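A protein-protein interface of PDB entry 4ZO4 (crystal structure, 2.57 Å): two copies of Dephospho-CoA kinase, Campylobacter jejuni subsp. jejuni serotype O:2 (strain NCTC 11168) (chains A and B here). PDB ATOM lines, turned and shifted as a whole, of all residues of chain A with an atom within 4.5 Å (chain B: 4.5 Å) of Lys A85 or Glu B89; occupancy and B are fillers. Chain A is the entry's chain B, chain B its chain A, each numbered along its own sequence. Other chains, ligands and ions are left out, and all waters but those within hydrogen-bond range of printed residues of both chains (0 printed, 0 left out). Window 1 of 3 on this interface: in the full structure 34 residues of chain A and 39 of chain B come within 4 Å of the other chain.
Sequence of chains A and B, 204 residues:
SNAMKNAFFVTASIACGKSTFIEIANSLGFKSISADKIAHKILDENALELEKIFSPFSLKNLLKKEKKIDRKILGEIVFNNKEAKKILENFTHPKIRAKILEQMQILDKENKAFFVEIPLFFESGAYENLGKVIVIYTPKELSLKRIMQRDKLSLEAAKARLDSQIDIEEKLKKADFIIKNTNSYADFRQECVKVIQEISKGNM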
ATOM      1  N   VAL A  78     -15.728 -18.701 -18.405  1.00  0.00           N
ATOM      2  CA  VAL A  78     -16.461 -17.594 -19.050  1.00  0.00           C
ATOM      3  C   VAL A  78     -16.830 -17.871 -20.511  1.00  0.00           C
ATOM      4  O   VAL A  78     -17.847 -17.413 -21.020  1.00  0.00           O
ATOM      5  CB  VAL A  78     -15.597 -16.312 -18.977  1.00  0.00           C
ATOM      6  CG1 VAL A  78     -15.752 -15.468 -20.207  1.00  0.00           C
ATOM      7  CG2 VAL A  78     -15.925 -15.522 -17.713  1.00  0.00           C
ATOM      8  N   ASN A  80     -18.461 -19.077 -23.522  1.00  0.00           N
ATOM      9  CA  ASN A  80     -19.794 -19.629 -23.845  1.00  0.00           C
ATOM     10  C   ASN A  80     -20.739 -19.694 -22.630  1.00  0.00           C
ATOM     11  O   ASN A  80     -21.767 -20.420 -22.601  1.00  0.00           O
ATOM     12  CB  ASN A  80     -19.690 -20.999 -24.562  1.00  0.00           C
ATOM     13  CG  ASN A  80     -20.765 -21.178 -25.618  1.00  0.00           C
ATOM     14  OD1 ASN A  80     -20.914 -20.341 -26.498  1.00  0.00           O
ATOM     15  ND2 ASN A  80     -21.547 -22.241 -25.512  1.00  0.00           N
ATOM     16  N   ASN A  81     -20.407 -18.895 -21.631  1.00  0.00           N
ATOM     17  CA  ASN A  81     -21.249 -18.802 -20.471  1.00  0.00           C
ATOM     18  C   ASN A  81     -21.679 -17.363 -20.284  1.00  0.00           C
ATOM     19  O   ASN A  81     -20.916 -16.510 -19.838  1.00  0.00           O
ATOM     20  CB  ASN A  81     -20.529 -19.331 -19.253  1.00  0.00           C
ATOM     21  CG  ASN A  81     -21.480 -19.651 -18.147  1.00  0.00           C
ATOM     22  OD1 ASN A  81     -22.205 -18.770 -17.670  1.00  0.00           O
ATOM     23  ND2 ASN A  81     -21.508 -20.912 -17.742  1.00  0.00           N
ATOM     24  N   LYS A  82     -22.916 -17.096 -20.658  1.00  0.00           N
ATOM     25  CA  LYS A  82     -23.437 -15.762 -20.649  1.00  0.00           C
ATOM     26  C   LYS A  82     -23.414 -15.118 -19.249  1.00  0.00           C
ATOM     27  O   LYS A  82     -23.325 -13.910 -19.125  1.00  0.00           O
ATOM     28  CB  LYS A  82     -24.868 -15.816 -21.186  1.00  0.00           C
ATOM     29  CG  LYS A  82     -25.502 -14.453 -21.365  1.00  0.00           C
ATOM     30  CD  LYS A  82     -26.982 -14.569 -21.674  1.00  0.00           C
ATOM     31  CE  LYS A  82     -27.565 -13.202 -21.990  1.00  0.00           C
ATOM     32  NZ  LYS A  82     -28.987 -13.146 -21.562  1.00  0.00           N
ATOM     33  N   GLU A  83     -23.538 -15.921 -18.199  1.00  0.00           N
ATOM     34  CA  GLU A  83     -23.754 -15.382 -16.873  1.00  0.00           C
ATOM     35  C   GLU A  83     -22.413 -15.083 -16.220  1.00  0.00           C
ATOM     36  O   GLU A  83     -22.230 -14.025 -15.583  1.00  0.00           O
ATOM     37  CB  GLU A  83     -24.585 -16.369 -16.069  1.00  0.00           C
ATOM     38  CG  GLU A  83     -24.806 -16.018 -14.617  1.00  0.00           C
ATOM     39  CD  GLU A  83     -25.783 -14.895 -14.451  1.00  0.00           C
ATOM     40  OE1 GLU A  83     -25.848 -14.319 -13.346  1.00  0.00           O
ATOM     41  OE2 GLU A  83     -26.466 -14.594 -15.440  1.00  0.00           O
ATOM     42  N   ALA A  84     -21.468 -16.003 -16.387  1.00  0.00           N
ATOM     43  CA  ALA A  84     -20.174 -15.802 -15.835  1.00  0.00           C
ATOM     44  C   ALA A  84     -19.539 -14.577 -16.439  1.00  0.00           C
ATOM     45  O   ALA A  84     -18.951 -13.813 -15.698  1.00  0.00           O
ATOM     46  CB  ALA A  84     -19.302 -17.025 -16.056  1.00  0.00           C
ATOM     47  N   LYS A  85     -19.674 -14.381 -17.761  1.00  0.00           N
ATOM     48  CA  LYS A  85     -19.236 -13.143 -18.451  1.00  0.00           C
ATOM     49  C   LYS A  85     -19.816 -11.897 -17.813  1.00  0.00           C
ATOM     50  O   LYS A  85     -19.105 -10.967 -17.489  1.00  0.00           O
ATOM     51  CB  LYS A  85     -19.676 -13.135 -19.914  1.00  0.00           C
ATOM     52  CG  LYS A  85     -18.893 -14.051 -20.841  1.00  0.00           C
ATOM     53  CD  LYS A  85     -19.477 -14.039 -22.259  1.00  0.00           C
ATOM     54  CE  LYS A  85     -19.168 -15.337 -23.004  1.00  0.00           C
ATOM     55  NZ  LYS A  85     -19.639 -15.324 -24.421  1.00  0.00           N
ATOM     56  N   LYS A  86     -21.127 -11.860 -17.661  1.00  0.00           N
ATOM     57  CA  LYS A  86     -21.787 -10.681 -17.096  1.00  0.00           C
ATOM     58  C   LYS A  86     -21.279 -10.386 -15.709  1.00  0.00           C
ATOM     59  O   LYS A  86     -20.985  -9.243 -15.419  1.00  0.00           O
ATOM     60  CB  LYS A  86     -23.308 -10.887 -17.067  1.00  0.00           C
ATOM     61  CG  LYS A  86     -24.102  -9.922 -16.198  1.00  0.00           C
ATOM     62  CD  LYS A  86     -25.309 -10.596 -15.519  1.00  0.00           C
ATOM     63  CE  LYS A  86     -26.649 -10.171 -16.111  1.00  0.00           C
ATOM     64  NZ  LYS A  86     -27.721 -11.179 -15.840  1.00  0.00           N
ATOM     65  N   ILE A  87     -21.185 -11.414 -14.846  1.00  0.00           N
ATOM     66  CA  ILE A  87     -20.740 -11.236 -13.449  1.00  0.00           C
ATOM     67  C   ILE A  87     -19.305 -10.703 -13.428  1.00  0.00           C
ATOM     68  O   ILE A  87     -18.965  -9.765 -12.695  1.00  0.00           O
ATOM     69  CB  ILE A  87     -20.879 -12.581 -12.677  1.00  0.00           C
ATOM     70  CG1 ILE A  87     -22.360 -12.994 -12.578  1.00  0.00           C
ATOM     71  CG2 ILE A  87     -20.246 -12.531 -11.285  1.00  0.00           C
ATOM     72  CD1 ILE A  87     -23.315 -11.869 -12.190  1.00  0.00           C
ATOM     73  N   LEU A  88     -18.468 -11.255 -14.296  1.00  0.00           N
ATOM     74  CA  LEU A  88     -17.052 -10.879 -14.361  1.00  0.00           C
ATOM     75  C   LEU A  88     -16.877  -9.453 -14.856  1.00  0.00           C
ATOM     76  O   LEU A  88     -16.130  -8.674 -14.294  1.00  0.00           O
ATOM     77  CB  LEU A  88     -16.296 -11.851 -15.279  1.00  0.00           C
ATOM     78  CG  LEU A  88     -14.800 -11.583 -15.462  1.00  0.00           C
ATOM     79  CD1 LEU A  88     -14.063 -11.464 -14.136  1.00  0.00           C
ATOM     80  CD2 LEU A  88     -14.193 -12.688 -16.320  1.00  0.00           C
ATOM     81  N   GLU A  89     -17.591  -9.122 -15.921  1.00  0.00           N
ATOM     82  CA  GLU A  89     -17.600  -7.795 -16.460  1.00  0.00           C
ATOM     83  C   GLU A  89     -18.176  -6.817 -15.454  1.00  0.00           C
ATOM     84  O   GLU A  89     -17.538  -5.848 -15.092  1.00  0.00           O
ATOM     85  CB  GLU A  89     -18.397  -7.768 -17.746  1.00  0.00           C
ATOM     86  CG  GLU A  89     -17.737  -8.530 -18.882  1.00  0.00           C
ATOM     87  CD  GLU A  89     -18.674  -8.742 -20.042  1.00  0.00           C
ATOM     88  OE1 GLU A  89     -19.803  -8.213 -19.973  1.00  0.00           O
ATOM     89  OE2 GLU A  89     -18.285  -9.425 -21.017  1.00  0.00           O
ATOM     90  N   LYS B  85     -14.776 -10.622 -28.643  1.00  0.00           N
ATOM     91  CA  LYS B  85     -15.766 -11.398 -27.956  1.00  0.00           C
ATOM     92  C   LYS B  85     -16.958 -11.690 -28.847  1.00  0.00           C
ATOM     93  O   LYS B  85     -17.407 -12.831 -28.925  1.00  0.00           O
ATOM     94  CB  LYS B  85     -16.239 -10.660 -26.709  1.00  0.00           C
ATOM     95  CG  LYS B  85     -16.935 -11.545 -25.677  1.00  0.00           C
ATOM     96  CD  LYS B  85     -17.998 -10.783 -24.906  1.00  0.00           C
ATOM     97  CE  LYS B  85     -17.496  -9.457 -24.341  1.00  0.00           C
ATOM     98  NZ  LYS B  85     -18.565  -8.700 -23.625  1.00  0.00           N
ATOM     99  N   LYS B  86     -17.505 -10.678 -29.514  1.00  0.00           N
ATOM    100  CA  LYS B  86     -18.690 -10.934 -30.325  1.00  0.00           C
ATOM    101  C   LYS B  86     -18.324 -11.857 -31.463  1.00  0.00           C
ATOM    102  O   LYS B  86     -19.066 -12.764 -31.786  1.00  0.00           O
ATOM    103  CB  LYS B  86     -19.317  -9.660 -30.845  1.00  0.00           C
ATOM    104  CG  LYS B  86     -19.996  -8.830 -29.768  1.00  0.00           C
ATOM    105  CD  LYS B  86     -20.745  -7.638 -30.356  1.00  0.00           C
ATOM    106  CE  LYS B  86     -21.245  -6.696 -29.250  1.00  0.00           C
ATOM    107  NZ  LYS B  86     -22.267  -5.691 -29.691  1.00  0.00           N
ATOM    108  N   ILE B  87     -17.155 -11.677 -32.057  1.00  0.00           N
ATOM    109  CA  ILE B  87     -16.804 -12.526 -33.180  1.00  0.00           C
ATOM    110  C   ILE B  87     -16.714 -13.974 -32.707  1.00  0.00           C
ATOM    111  O   ILE B  87     -17.255 -14.882 -33.360  1.00  0.00           O
ATOM    112  CB  ILE B  87     -15.530 -12.039 -33.880  1.00  0.00           C
ATOM    113  CG1 ILE B  87     -15.796 -10.717 -34.605  1.00  0.00           C
ATOM    114  CG2 ILE B  87     -15.098 -12.997 -34.964  1.00  0.00           C
ATOM    115  CD1 ILE B  87     -14.535 -10.068 -35.125  1.00  0.00           C
ATOM    116  N   LEU B  88     -16.077 -14.196 -31.555  1.00  0.00           N
ATOM    117  CA  LEU B  88     -15.946 -15.539 -31.045  1.00  0.00           C
ATOM    118  C   LEU B  88     -17.327 -16.188 -30.800  1.00  0.00           C
ATOM    119  O   LEU B  88     -17.608 -17.308 -31.267  1.00  0.00           O
ATOM    120  CB  LEU B  88     -15.134 -15.556 -29.770  1.00  0.00           C
ATOM    121  CG  LEU B  88     -14.677 -16.991 -29.467  1.00  0.00           C
ATOM    122  CD1 LEU B  88     -13.762 -17.521 -30.565  1.00  0.00           C
ATOM    123  CD2 LEU B  88     -13.989 -17.031 -28.107  1.00  0.00           C
ATOM    124  N   GLU B  89     -18.192 -15.469 -30.099  1.00  0.00           N
ATOM    125  CA  GLU B  89     -19.547 -15.948 -29.880  1.00  0.00           C
ATOM    126  C   GLU B  89     -20.199 -16.356 -31.199  1.00  0.00           C
ATOM    127  O   GLU B  89     -20.701 -17.459 -31.299  1.00  0.00           O
ATOM    128  CB  GLU B  89     -20.405 -14.899 -29.175  1.00  0.00           C
ATOM    129  CG  GLU B  89     -20.024 -14.651 -27.713  1.00  0.00           C
ATOM    130  CD  GLU B  89     -20.546 -13.310 -27.159  1.00  0.00           C
ATOM    131  OE1 GLU B  89     -21.197 -12.528 -27.916  1.00  0.00           O
ATOM    132  OE2 GLU B  89     -20.285 -13.008 -25.963  1.00  0.00           O
ATOM    133  N   ASN B  90     -20.160 -15.505 -32.219  1.00  0.00           N
ATOM    134  CA  ASN B  90     -20.846 -15.811 -33.462  1.00  0.00           C
ATOM    135  C   ASN B  90     -20.105 -16.874 -34.237  1.00  0.00           C
ATOM    136  O   ASN B  90     -20.681 -17.673 -34.983  1.00  0.00           O
ATOM    137  CB  ASN B  90     -21.014 -14.559 -34.302  1.00  0.00           C
ATOM    138  CG  ASN B  90     -21.578 -14.859 -35.667  1.00  0.00           C
ATOM    139  OD1 ASN B  90     -22.770 -15.082 -35.814  1.00  0.00           O
ATOM    140  ND2 ASN B  90     -20.720 -14.871 -36.673  1.00  0.00           N
ATOM    141  N   PHE B  91     -18.808 -16.930 -34.041  1.00  0.00           N
ATOM    142  CA  PHE B  91     -18.044 -18.019 -34.643  1.00  0.00           C
ATOM    143  C   PHE B  91     -18.415 -19.390 -34.115  1.00  0.00           C
ATOM    144  O   PHE B  91     -18.498 -20.321 -34.898  1.00  0.00           O
ATOM    145  CB  PHE B  91     -16.564 -17.808 -34.410  1.00  0.00           C
ATOM    146  CG  PHE B  91     -15.698 -18.687 -35.245  1.00  0.00           C
ATOM    147  CD1 PHE B  91     -15.521 -18.435 -36.595  1.00  0.00           C
ATOM    148  CD2 PHE B  91     -15.027 -19.741 -34.675  1.00  0.00           C
ATOM    149  CE1 PHE B  91     -14.686 -19.250 -37.365  1.00  0.00           C
ATOM    150  CE2 PHE B  91     -14.207 -20.563 -35.419  1.00  0.00           C
ATOM    151  CZ  PHE B  91     -14.019 -20.310 -36.760  1.00  0.00           C
ATOM    152  N   THR B  92     -18.593 -19.511 -32.792  1.00  0.00           N
ATOM    153  CA  THR B  92     -18.646 -20.810 -32.119  1.00  0.00           C
ATOM    154  C   THR B  92     -20.065 -21.338 -31.968  1.00  0.00           C
ATOM    155  O   THR B  92     -20.316 -22.510 -32.131  1.00  0.00           O
ATOM    156  CB  THR B  92     -18.057 -20.722 -30.701  1.00  0.00           C
ATOM    157  OG1 THR B  92     -18.653 -19.634 -29.996  1.00  0.00           O
ATOM    158  CG2 THR B  92     -16.577 -20.498 -30.746  1.00  0.00           C
ATOM    159  N   HIS B  93     -20.991 -20.449 -31.635  1.00  0.00           N
ATOM    160  CA  HIS B  93     -22.366 -20.825 -31.363  1.00  0.00           C
ATOM    161  C   HIS B  93     -22.970 -21.812 -32.365  1.00  0.00           C
ATOM    162  O   HIS B  93     -23.472 -22.857 -31.952  1.00  0.00           O
ATOM    163  CB  HIS B  93     -23.276 -19.601 -31.225  1.00  0.00           C
ATOM    164  CG  HIS B  93     -23.054 -18.798 -29.979  1.00  0.00           C
ATOM    165  ND1 HIS B  93     -23.668 -17.577 -29.763  1.00  0.00           N
ATOM    166  CD2 HIS B  93     -22.292 -19.031 -28.885  1.00  0.00           C
ATOM    167  CE1 HIS B  93     -23.315 -17.115 -28.575  1.00  0.00           C
ATOM    168  NE2 HIS B  93     -22.465 -17.966 -28.029  1.00  0.00           N
ATOM    169  N   GLU B 123     -24.715 -21.100 -23.988  1.00  0.00           N
ATOM    170  CA  GLU B 123     -25.093 -20.092 -24.937  1.00  0.00           C
ATOM    171  C   GLU B 123     -25.690 -20.595 -26.243  1.00  0.00           C
ATOM    172  O   GLU B 123     -26.681 -20.042 -26.732  1.00  0.00           O
ATOM    173  CB  GLU B 123     -23.862 -19.246 -25.259  1.00  0.00           C
ATOM    174  CG  GLU B 123     -23.526 -18.208 -24.207  1.00  0.00           C
ATOM    175  CD  GLU B 123     -22.450 -17.225 -24.658  1.00  0.00           C
ATOM    176  OE1 GLU B 123     -21.808 -17.444 -25.716  1.00  0.00           O
ATOM    177  OE2 GLU B 123     -22.238 -16.226 -23.946  1.00  0.00           O
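NZ of Lys B85 lies within salt-bridge range of OE2 of Glu A89 (2.7 Å). The side-chain carboxylate (OE2) of Glu B89 lies within salt-bridge range of the side-chain amino group (NZ) of Lys A85 (2.9 Å). The backbone NH (N) of Lys A82 is in hydrogen-bond range of the side-chain carboxylate (OE2) of Glu B123, at 3.5 Å. The side-chain amide oxygen (OD1) of Asn A80 sits close to the side-chain carboxylate (OE1) of Glu B123 (3.1 Å). A ring nitrogen (NE2) of His B93 sits close to the side-chain amide oxygen (OD1) of Asn A80 (3.2 Å). The side-chain carboxylate of Glu B123 lies within salt-bridge range of the side-chain amino group of Lys A85.
The side-chain amide oxygen (OD1) of Asn A81 is in hydrogen-bond range of the backbone NH (N) of Ala A84, at 3.1 Å. The side-chain carboxylate of Glu B123 is in hydrogen-bond range of a ring nitrogen (NE2) of His B93. The backbone carbonyl oxygen (O) of Glu B89 lies close to a ring nitrogen (ND1) of His B93, 3.3 Å away. O of Glu B89 sits at hydrogen-bond distance from OG1 of Thr B92. OD1 of Asn A81 lies close to N of Glu A83.
Asn A81 touches Glu B123.
Of chain B, only Glu B89 and Glu B123 come within 4 Å of Lys A85. Glu B89 touches just one residue of chain A: Lys A85. Printed residues of chain A within 4 Å of Glu B123: Asn A80, Asn A81, Lys A82 and Lys A85. Printed residues of chain A within 4 Å of His B93: Asn A80 (3.1 Å). Printed residues of chain A within 4 Å of Lys B85: Glu A89. Of the printed residues of chain B, Glu A89 touches Lys B85 (2.7 Å). Of the printed residues of chain B, Asn A81 touches Glu B123 (3.9 Å). The nearest printed residue of chain A that does not touch Glu B89 is Asn A80 (5.6 Å).
Of the 11 printed residues of chain A, 5 touch a printed residue of chain B. Among the printed residues, Asp or Glu carboxylates within 4 Å of a Lys or Arg side-chain nitrogen of the other chain: Lys A85 with Glu B89, Lys A85 with Glu B123 and Glu A89 with Lys B85.
Lys A85 touches Glu B89, and with the chains exchanged Glu A89 touches Lys B85.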
